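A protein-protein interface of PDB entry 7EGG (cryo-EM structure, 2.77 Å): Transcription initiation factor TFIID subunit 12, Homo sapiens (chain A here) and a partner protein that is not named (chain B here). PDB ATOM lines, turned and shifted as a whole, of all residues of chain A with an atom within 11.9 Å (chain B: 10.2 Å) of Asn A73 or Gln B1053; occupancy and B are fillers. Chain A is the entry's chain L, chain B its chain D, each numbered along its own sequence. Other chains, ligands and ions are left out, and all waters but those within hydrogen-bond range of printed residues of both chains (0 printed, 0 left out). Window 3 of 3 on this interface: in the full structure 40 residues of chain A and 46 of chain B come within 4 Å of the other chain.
Among the printed residues, pairs that only touch across the chains: Gln A75 with Arg B1057, Glu A74 with Thr B1056, Asn A73 with Ile B1055, Glu A74 with Val B1058, Leu A76 with Val B1058, Glu A74 with Gln B922, Gln A75 with Ile B1055 and Asn A73 with Thr B1056.
Of chain B, only Ser B918 (3.3 Å) and Gln B922 (2.4 Å) come within 4 Å of Asp A71. Of the printed residues of chain B, Gln A75 touches Ile B1055, Thr B1056, Arg B1057 and Val B1058. Printed residues of chain B within 4 Å of Asp A77: Arg B1057 (2.6 Å) and Val B1058 (3.0 Å). Printed residues of chain A within 4 Å of Ser B918: Asp A71 (3.3 Å) and Glu A74 (2.4 Å). Gln B1053 touches one residue of chain A. Of the printed residues of chain A, Arg B1054 touches Asn A73. Ile B1055 touches just these residues of chain A: Asn A73 and Gln A75. The nearest residue of chain B that does not touch Asn A73 is Gln B922 (5.6 Å). The nearest residue of chain A that does not touch Gln B1053 is Pro A72 (7.6 Å). The nearest printed residue of chain B that does not touch Gln A75 is Ala B921 (7.4 Å).
The backbone carbonyl oxygen of Arg B1054 is in hydrogen-bond range of the side-chain amide nitrogen of Asn A73, at 2.6 Å. O of Val B1058 sits at hydrogen-bond distance from N of Asp A77 (3.4 Å). The side-chain hydroxyl (OG) of Ser B918 lies within hydrogen-bond range of the side-chain carboxylate (OD1) of Asp A71. OD1 of Asp A77 lies within salt-bridge range of NH2 of Arg B1057. The backbone NH (N) of Gln A75 lies within hydrogen-bond range of the backbone carbonyl oxygen (O) of Thr B1056 (3.1 Å). The side-chain hydroxyl (OG) of Ser B918 sits close to the side-chain carboxylate (OE2) of Glu A74 (3.3 Å). NE2 of Gln B922 sits at hydrogen-bond distance from OD2 of Asp A71, 2.4 Å away. ND2 of Asn A73 sits close to NE2 of Gln B1053, at 3.2 Å. N of Val B1058 sits at hydrogen-bond distance from O of Gln A75 (3.3 Å).
The backbone carbonyl oxygen (O) of Glu B858 sits close to the side-chain amide oxygen (OE1) of Gln B922, 3.4 Å away. O of Arg B1057 sits at hydrogen-bond distance from NZ of Lys B924 (2.7 Å).
Hydrophobic or aromatic side chains of chain B that line the printed part of chain A: Ile B1055 and Val B1058. Of the 15 printed residues of chain A, 6 touch a printed residue of chain B. Along chain A the printed residues that touch a printed residue of chain B span positions 71 to 77. Among the printed residues, 17 pairs touch across the chains.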
ATOM      1  N   LEU A  63     -25.778  -6.466  -2.603  1.00  0.00           N
ATOM      2  CA  LEU A  63     -25.530  -5.124  -3.114  1.00  0.00           C
ATOM      3  C   LEU A  63     -24.558  -4.370  -2.217  1.00  0.00           C
ATOM      4  O   LEU A  63     -23.747  -3.573  -2.702  1.00  0.00           O
ATOM      5  CB  LEU A  63     -26.847  -4.362  -3.240  1.00  0.00           C
ATOM      6  CG  LEU A  63     -26.794  -2.997  -3.922  1.00  0.00           C
ATOM      7  CD1 LEU A  63     -26.498  -3.141  -5.402  1.00  0.00           C
ATOM      8  CD2 LEU A  63     -28.091  -2.263  -3.705  1.00  0.00           C
ATOM      9  N   GLN A  64     -24.616  -4.614  -0.906  1.00  0.00           N
ATOM     10  CA  GLN A  64     -23.666  -3.999   0.010  1.00  0.00           C
ATOM     11  C   GLN A  64     -22.275  -4.601  -0.120  1.00  0.00           C
ATOM     12  O   GLN A  64     -21.294  -3.948   0.251  1.00  0.00           O
ATOM     13  CB  GLN A  64     -24.157  -4.134   1.450  1.00  0.00           C
ATOM     14  CG  GLN A  64     -25.421  -3.348   1.749  1.00  0.00           C
ATOM     15  CD  GLN A  64     -25.878  -3.513   3.181  1.00  0.00           C
ATOM     16  OE1 GLN A  64     -25.268  -4.246   3.959  1.00  0.00           O
ATOM     17  NE2 GLN A  64     -26.961  -2.832   3.539  1.00  0.00           N
ATOM     18  N   ASP A  65     -22.164  -5.827  -0.632  1.00  0.00           N
ATOM     19  CA  ASP A  65     -20.860  -6.380  -0.958  1.00  0.00           C
ATOM     20  C   ASP A  65     -20.337  -5.867  -2.290  1.00  0.00           C
ATOM     21  O   ASP A  65     -19.128  -5.929  -2.533  1.00  0.00           O
ATOM     22  CB  ASP A  65     -20.919  -7.909  -0.976  1.00  0.00           C
ATOM     23  CG  ASP A  65     -21.106  -8.501   0.407  1.00  0.00           C
ATOM     24  OD1 ASP A  65     -20.673  -7.866   1.392  1.00  0.00           O
ATOM     25  OD2 ASP A  65     -21.679  -9.606   0.510  1.00  0.00           O
ATOM     26  N   LEU A  66     -21.220  -5.365  -3.157  1.00  0.00           N
ATOM     27  CA  LEU A  66     -20.772  -4.683  -4.363  1.00  0.00           C
ATOM     28  C   LEU A  66     -20.182  -3.316  -4.055  1.00  0.00           C
ATOM     29  O   LEU A  66     -19.394  -2.798  -4.852  1.00  0.00           O
ATOM     30  CB  LEU A  66     -21.928  -4.537  -5.349  1.00  0.00           C
ATOM     31  CG  LEU A  66     -21.544  -4.437  -6.825  1.00  0.00           C
ATOM     32  CD1 LEU A  66     -21.038  -5.773  -7.329  1.00  0.00           C
ATOM     33  CD2 LEU A  66     -22.721  -3.962  -7.651  1.00  0.00           C
ATOM     34  N   VAL A  67     -20.547  -2.724  -2.922  1.00  0.00           N
ATOM     35  CA  VAL A  67     -19.964  -1.457  -2.509  1.00  0.00           C
ATOM     36  C   VAL A  67     -18.693  -1.672  -1.690  1.00  0.00           C
ATOM     37  O   VAL A  67     -17.739  -0.900  -1.825  1.00  0.00           O
ATOM     38  CB  VAL A  67     -21.010  -0.641  -1.731  1.00  0.00           C
ATOM     39  CG1 VAL A  67     -20.501   0.756  -1.405  1.00  0.00           C
ATOM     40  CG2 VAL A  67     -22.290  -0.563  -2.526  1.00  0.00           C
ATOM     41  N   ARG A  68     -18.651  -2.731  -0.872  1.00  0.00           N
ATOM     42  CA  ARG A  68     -17.468  -3.030  -0.067  1.00  0.00           C
ATOM     43  C   ARG A  68     -16.270  -3.412  -0.926  1.00  0.00           C
ATOM     44  O   ARG A  68     -15.125  -3.170  -0.529  1.00  0.00           O
ATOM     45  CB  ARG A  68     -17.765  -4.157   0.921  1.00  0.00           C
ATOM     46  CG  ARG A  68     -18.539  -3.738   2.155  1.00  0.00           C
ATOM     47  CD  ARG A  68     -18.852  -4.947   3.022  1.00  0.00           C
ATOM     48  NE  ARG A  68     -19.735  -4.617   4.136  1.00  0.00           N
ATOM     49  CZ  ARG A  68     -20.512  -5.500   4.755  1.00  0.00           C
ATOM     50  NH1 ARG A  68     -20.516  -6.768   4.367  1.00  0.00           N
ATOM     51  NH2 ARG A  68     -21.286  -5.118   5.761  1.00  0.00           N
ATOM     52  N   GLU A  69     -16.509  -4.016  -2.091  1.00  0.00           N
ATOM     53  CA  GLU A  69     -15.413  -4.350  -2.993  1.00  0.00           C
ATOM     54  C   GLU A  69     -14.807  -3.101  -3.623  1.00  0.00           C
ATOM     55  O   GLU A  69     -13.592  -3.045  -3.843  1.00  0.00           O
ATOM     56  CB  GLU A  69     -15.909  -5.318  -4.070  1.00  0.00           C
ATOM     57  CG  GLU A  69     -14.843  -5.817  -5.036  1.00  0.00           C
ATOM     58  CD  GLU A  69     -13.828  -6.731  -4.381  1.00  0.00           C
ATOM     59  OE1 GLU A  69     -14.179  -7.408  -3.391  1.00  0.00           O
ATOM     60  OE2 GLU A  69     -12.672  -6.770  -4.855  1.00  0.00           O
ATOM     61  N   VAL A  70     -15.626  -2.087  -3.897  1.00  0.00           N
ATOM     62  CA  VAL A  70     -15.108  -0.843  -4.456  1.00  0.00           C
ATOM     63  C   VAL A  70     -14.444  -0.002  -3.370  1.00  0.00           C
ATOM     64  O   VAL A  70     -13.254   0.321  -3.454  1.00  0.00           O
ATOM     65  CB  VAL A  70     -16.230  -0.068  -5.171  1.00  0.00           C
ATOM     66  CG1 VAL A  70     -15.662   1.152  -5.865  1.00  0.00           C
ATOM     67  CG2 VAL A  70     -16.939  -0.966  -6.167  1.00  0.00           C
ATOM     68  N   ASP A  71     -15.198   0.357  -2.332  1.00  0.00           N
ATOM     69  CA  ASP A  71     -14.657   1.083  -1.184  1.00  0.00           C
ATOM     70  C   ASP A  71     -14.936   0.288   0.082  1.00  0.00           C
ATOM     71  O   ASP A  71     -16.112  -0.013   0.374  1.00  0.00           O
ATOM     72  CB  ASP A  71     -15.250   2.489  -1.053  1.00  0.00           C
ATOM     73  CG  ASP A  71     -14.989   3.352  -2.260  1.00  0.00           C
ATOM     74  OD1 ASP A  71     -15.653   3.148  -3.292  1.00  0.00           O
ATOM     75  OD2 ASP A  71     -14.138   4.258  -2.163  1.00  0.00           O
ATOM     76  N   PRO A  72     -13.917  -0.051   0.876  1.00  0.00           N
ATOM     77  CA  PRO A  72     -14.183  -0.692   2.172  1.00  0.00           C
ATOM     78  C   PRO A  72     -14.825   0.240   3.184  1.00  0.00           C
ATOM     79  O   PRO A  72     -15.407  -0.241   4.162  1.00  0.00           O
ATOM     80  CB  PRO A  72     -12.791  -1.148   2.637  1.00  0.00           C
ATOM     81  CG  PRO A  72     -11.901  -1.025   1.432  1.00  0.00           C
ATOM     82  CD  PRO A  72     -12.475   0.089   0.622  1.00  0.00           C
ATOM     83  N   ASN A  73     -14.740   1.552   2.980  1.00  0.00           N
ATOM     84  CA  ASN A  73     -15.352   2.546   3.854  1.00  0.00           C
ATOM     85  C   ASN A  73     -16.336   3.358   3.017  1.00  0.00           C
ATOM     86  O   ASN A  73     -15.997   4.435   2.523  1.00  0.00           O
ATOM     87  CB  ASN A  73     -14.287   3.440   4.475  1.00  0.00           C
ATOM     88  CG  ASN A  73     -14.832   4.305   5.590  1.00  0.00           C
ATOM     89  OD1 ASN A  73     -15.991   4.182   5.987  1.00  0.00           O
ATOM     90  ND2 ASN A  73     -14.005   5.217   6.083  1.00  0.00           N
ATOM     91  N   GLU A  74     -17.559   2.845   2.878  1.00  0.00           N
ATOM     92  CA  GLU A  74     -18.629   3.560   2.197  1.00  0.00           C
ATOM     93  C   GLU A  74     -19.960   2.962   2.622  1.00  0.00           C
ATOM     94  O   GLU A  74     -20.088   1.742   2.741  1.00  0.00           O
ATOM     95  CB  GLU A  74     -18.489   3.497   0.672  1.00  0.00           C
ATOM     96  CG  GLU A  74     -19.311   4.549  -0.055  1.00  0.00           C
ATOM     97  CD  GLU A  74     -18.843   4.781  -1.475  1.00  0.00           C
ATOM     98  OE1 GLU A  74     -19.414   4.170  -2.401  1.00  0.00           O
ATOM     99  OE2 GLU A  74     -17.896   5.572  -1.663  1.00  0.00           O
ATOM    100  N   GLN A  75     -20.944   3.829   2.853  1.00  0.00           N
ATOM    101  CA  GLN A  75     -22.286   3.421   3.241  1.00  0.00           C
ATOM    102  C   GLN A  75     -23.298   4.164   2.386  1.00  0.00           C
ATOM    103  O   GLN A  75     -23.322   5.397   2.385  1.00  0.00           O
ATOM    104  CB  GLN A  75     -22.549   3.699   4.726  1.00  0.00           C
ATOM    105  CG  GLN A  75     -21.693   2.896   5.689  1.00  0.00           C
ATOM    106  CD  GLN A  75     -22.244   1.508   5.940  1.00  0.00           C
ATOM    107  OE1 GLN A  75     -23.398   1.221   5.622  1.00  0.00           O
ATOM    108  NE2 GLN A  75     -21.422   0.638   6.512  1.00  0.00           N
ATOM    109  N   LEU A  76     -24.129   3.420   1.665  1.00  0.00           N
ATOM    110  CA  LEU A  76     -25.193   4.040   0.895  1.00  0.00           C
ATOM    111  C   LEU A  76     -26.334   4.471   1.816  1.00  0.00           C
ATOM    112  O   LEU A  76     -26.385   4.128   2.998  1.00  0.00           O
ATOM    113  CB  LEU A  76     -25.722   3.081  -0.169  1.00  0.00           C
ATOM    114  CG  LEU A  76     -24.799   2.518  -1.249  1.00  0.00           C
ATOM    115  CD1 LEU A  76     -25.443   1.305  -1.885  1.00  0.00           C
ATOM    116  CD2 LEU A  76     -24.500   3.555  -2.305  1.00  0.00           C
ATOM    117  N   ASP A  77     -27.240   5.253   1.251  1.00  0.00           N
ATOM    118  CA  ASP A  77     -28.446   5.632   2.012  1.00  0.00           C
ATOM    119  C   ASP A  77     -29.507   4.598   1.653  1.00  0.00           C
ATOM    120  O   ASP A  77     -29.348   3.911   0.638  1.00  0.00           O
ATOM    121  CB  ASP A  77     -28.903   7.040   1.643  1.00  0.00           C
ATOM    122  CG  ASP A  77     -28.311   8.118   2.528  1.00  0.00           C
ATOM    123  OD1 ASP A  77     -28.550   8.063   3.747  1.00  0.00           O
ATOM    124  OD2 ASP A  77     -27.621   9.001   1.994  1.00  0.00           O
ATOM    125  N   THR B 855     -10.607   6.754  -7.258  1.00  0.00           N
ATOM    126  CA  THR B 855     -11.218   6.318  -6.007  1.00  0.00           C
ATOM    127  C   THR B 855     -10.186   5.675  -5.089  1.00  0.00           C
ATOM    128  O   THR B 855     -10.373   5.634  -3.867  1.00  0.00           O
ATOM    129  CB  THR B 855     -12.370   5.351  -6.278  1.00  0.00           C
ATOM    130  OG1 THR B 855     -11.960   4.366  -7.232  1.00  0.00           O
ATOM    131  CG2 THR B 855     -13.573   6.091  -6.824  1.00  0.00           C
ATOM    132  N   GLU B 858      -8.790   8.523  -3.344  1.00  0.00           N
ATOM    133  CA  GLU B 858      -9.821   9.106  -2.475  1.00  0.00           C
ATOM    134  C   GLU B 858     -10.266  10.508  -2.887  1.00  0.00           C
ATOM    135  O   GLU B 858     -11.316  10.982  -2.458  1.00  0.00           O
ATOM    136  CB  GLU B 858      -9.343   9.121  -1.019  1.00  0.00           C
ATOM    137  CG  GLU B 858      -9.199   7.739  -0.405  1.00  0.00           C
ATOM    138  CD  GLU B 858      -7.771   7.232  -0.439  1.00  0.00           C
ATOM    139  OE1 GLU B 858      -6.854   8.048  -0.667  1.00  0.00           O
ATOM    140  OE2 GLU B 858      -7.567   6.017  -0.241  1.00  0.00           O
ATOM    141  N   SER B 918     -19.438   6.389  -6.572  1.00  0.00           N
ATOM    142  CA  SER B 918     -18.417   6.502  -5.539  1.00  0.00           C
ATOM    143  C   SER B 918     -17.385   7.571  -5.856  1.00  0.00           C
ATOM    144  O   SER B 918     -16.835   8.175  -4.932  1.00  0.00           O
ATOM    145  CB  SER B 918     -17.715   5.161  -5.335  1.00  0.00           C
ATOM    146  OG  SER B 918     -18.526   4.273  -4.593  1.00  0.00           O
ATOM    147  N   ALA B 921     -19.255  10.717  -4.863  1.00  0.00           N
ATOM    148  CA  ALA B 921     -19.471  10.836  -3.430  1.00  0.00           C
ATOM    149  C   ALA B 921     -18.186  11.151  -2.683  1.00  0.00           C
ATOM    150  O   ALA B 921     -18.247  11.599  -1.534  1.00  0.00           O
ATOM    151  CB  ALA B 921     -20.084   9.555  -2.865  1.00  0.00           C
ATOM    152  N   GLN B 922     -17.034  10.912  -3.298  1.00  0.00           N
ATOM    153  CA  GLN B 922     -15.756  11.352  -2.762  1.00  0.00           C
ATOM    154  C   GLN B 922     -15.314  12.683  -3.349  1.00  0.00           C
ATOM    155  O   GLN B 922     -14.278  13.214  -2.941  1.00  0.00           O
ATOM    156  CB  GLN B 922     -14.685  10.290  -3.012  1.00  0.00           C
ATOM    157  CG  GLN B 922     -14.938   8.993  -2.269  1.00  0.00           C
ATOM    158  CD  GLN B 922     -13.997   7.889  -2.689  1.00  0.00           C
ATOM    159  OE1 GLN B 922     -12.969   8.139  -3.312  1.00  0.00           O
ATOM    160  NE2 GLN B 922     -14.350   6.655  -2.353  1.00  0.00           N
ATOM    161  N   LYS B 924     -17.094  15.351  -2.912  1.00  0.00           N
ATOM    162  CA  LYS B 924     -17.494  16.288  -1.873  1.00  0.00           C
ATOM    163  C   LYS B 924     -16.639  16.186  -0.620  1.00  0.00           C
ATOM    164  O   LYS B 924     -16.684  17.095   0.214  1.00  0.00           O
ATOM    165  CB  LYS B 924     -18.963  16.067  -1.502  1.00  0.00           C
ATOM    166  CG  LYS B 924     -19.247  14.714  -0.864  1.00  0.00           C
ATOM    167  CD  LYS B 924     -20.709  14.579  -0.466  1.00  0.00           C
ATOM    168  CE  LYS B 924     -20.939  13.351   0.403  1.00  0.00           C
ATOM    169  NZ  LYS B 924     -20.839  12.082  -0.368  1.00  0.00           N
ATOM    170  N   ASN B 925     -15.863  15.112  -0.465  1.00  0.00           N
ATOM    171  CA  ASN B 925     -15.013  14.923   0.704  1.00  0.00           C
ATOM    172  C   ASN B 925     -13.578  15.373   0.458  1.00  0.00           C
ATOM    173  O   ASN B 925     -12.651  14.863   1.094  1.00  0.00           O
ATOM    174  CB  ASN B 925     -15.041  13.463   1.154  1.00  0.00           C
ATOM    175  CG  ASN B 925     -16.400  13.041   1.671  1.00  0.00           C
ATOM    176  OD1 ASN B 925     -17.057  12.177   1.093  1.00  0.00           O
ATOM    177  ND2 ASN B 925     -16.830  13.655   2.765  1.00  0.00           N
ATOM    178  N   GLN B1053     -12.611   7.819  11.816  1.00  0.00           N
ATOM    179  CA  GLN B1053     -12.749   7.242  10.484  1.00  0.00           C
ATOM    180  C   GLN B1053     -13.875   7.915   9.710  1.00  0.00           C
ATOM    181  O   GLN B1053     -15.047   7.771  10.056  1.00  0.00           O
ATOM    182  CB  GLN B1053     -13.001   5.737  10.574  1.00  0.00           C
ATOM    183  CG  GLN B1053     -12.874   5.012   9.248  1.00  0.00           C
ATOM    184  CD  GLN B1053     -11.438   4.902   8.781  1.00  0.00           C
ATOM    185  OE1 GLN B1053     -10.565   4.449   9.522  1.00  0.00           O
ATOM    186  NE2 GLN B1053     -11.180   5.328   7.550  1.00  0.00           N
ATOM    187  N   ARG B1054     -13.511   8.651   8.663  1.00  0.00           N
ATOM    188  CA  ARG B1054     -14.490   9.349   7.837  1.00  0.00           C
ATOM    189  C   ARG B1054     -15.225   8.345   6.958  1.00  0.00           C
ATOM    190  O   ARG B1054     -14.630   7.739   6.061  1.00  0.00           O
ATOM    191  CB  ARG B1054     -13.802  10.418   6.990  1.00  0.00           C
ATOM    192  CG  ARG B1054     -13.629  11.758   7.694  1.00  0.00           C
ATOM    193  CD  ARG B1054     -12.252  11.888   8.329  1.00  0.00           C
ATOM    194  NE  ARG B1054     -12.079  13.173   9.002  1.00  0.00           N
ATOM    195  CZ  ARG B1054     -12.250  13.360  10.307  1.00  0.00           C
ATOM    196  NH1 ARG B1054     -12.600  12.345  11.085  1.00  0.00           N
ATOM    197  NH2 ARG B1054     -12.071  14.562  10.838  1.00  0.00           N
ATOM    198  N   ILE B1055     -16.516   8.165   7.213  1.00  0.00           N
ATOM    199  CA  ILE B1055     -17.350   7.261   6.431  1.00  0.00           C
ATOM    200  C   ILE B1055     -17.977   8.051   5.293  1.00  0.00           C
ATOM    201  O   ILE B1055     -18.782   8.959   5.527  1.00  0.00           O
ATOM    202  CB  ILE B1055     -18.431   6.603   7.302  1.00  0.00           C
ATOM    203  CG1 ILE B1055     -17.793   5.725   8.379  1.00  0.00           C
ATOM    204  CG2 ILE B1055     -19.378   5.786   6.442  1.00  0.00           C
ATOM    205  CD1 ILE B1055     -18.546   5.727   9.687  1.00  0.00           C
ATOM    206  N   THR B1056     -17.604   7.715   4.062  1.00  0.00           N
ATOM    207  CA  THR B1056     -18.175   8.381   2.900  1.00  0.00           C
ATOM    208  C   THR B1056     -19.595   7.882   2.674  1.00  0.00           C
ATOM    209  O   THR B1056     -19.825   6.676   2.555  1.00  0.00           O
ATOM    210  CB  THR B1056     -17.318   8.122   1.664  1.00  0.00           C
ATOM    211  OG1 THR B1056     -15.976   8.549   1.914  1.00  0.00           O
ATOM    212  CG2 THR B1056     -17.864   8.886   0.473  1.00  0.00           C
ATOM    213  N   ARG B1057     -20.549   8.804   2.620  1.00  0.00           N
ATOM    214  CA  ARG B1057     -21.957   8.461   2.500  1.00  0.00           C
ATOM    215  C   ARG B1057     -22.505   8.963   1.173  1.00  0.00           C
ATOM    216  O   ARG B1057     -22.347  10.139   0.827  1.00  0.00           O
ATOM    217  CB  ARG B1057     -22.769   9.041   3.659  1.00  0.00           C
ATOM    218  CG  ARG B1057     -22.343   8.523   5.022  1.00  0.00           C
ATOM    219  CD  ARG B1057     -23.475   8.617   6.028  1.00  0.00           C
ATOM    220  NE  ARG B1057     -24.736   8.141   5.468  1.00  0.00           N
ATOM    221  CZ  ARG B1057     -25.798   7.810   6.194  1.00  0.00           C
ATOM    222  NH1 ARG B1057     -25.752   7.899   7.516  1.00  0.00           N
ATOM    223  NH2 ARG B1057     -26.905   7.389   5.600  1.00  0.00           N
ATOM    224  N   VAL B1058     -23.152   8.068   0.441  1.00  0.00           N
ATOM    225  CA  VAL B1058     -23.678   8.372  -0.882  1.00  0.00           C
ATOM    226  C   VAL B1058     -25.125   8.820  -0.746  1.00  0.00           C
ATOM    227  O   VAL B1058     -25.981   8.062  -0.278  1.00  0.00           O
ATOM    228  CB  VAL B1058     -23.562   7.152  -1.808  1.00  0.00           C
ATOM    229  CG1 VAL B1058     -23.810   7.549  -3.248  1.00  0.00           C
ATOM    230  CG2 VAL B1058     -22.197   6.504  -1.654  1.00  0.00           C
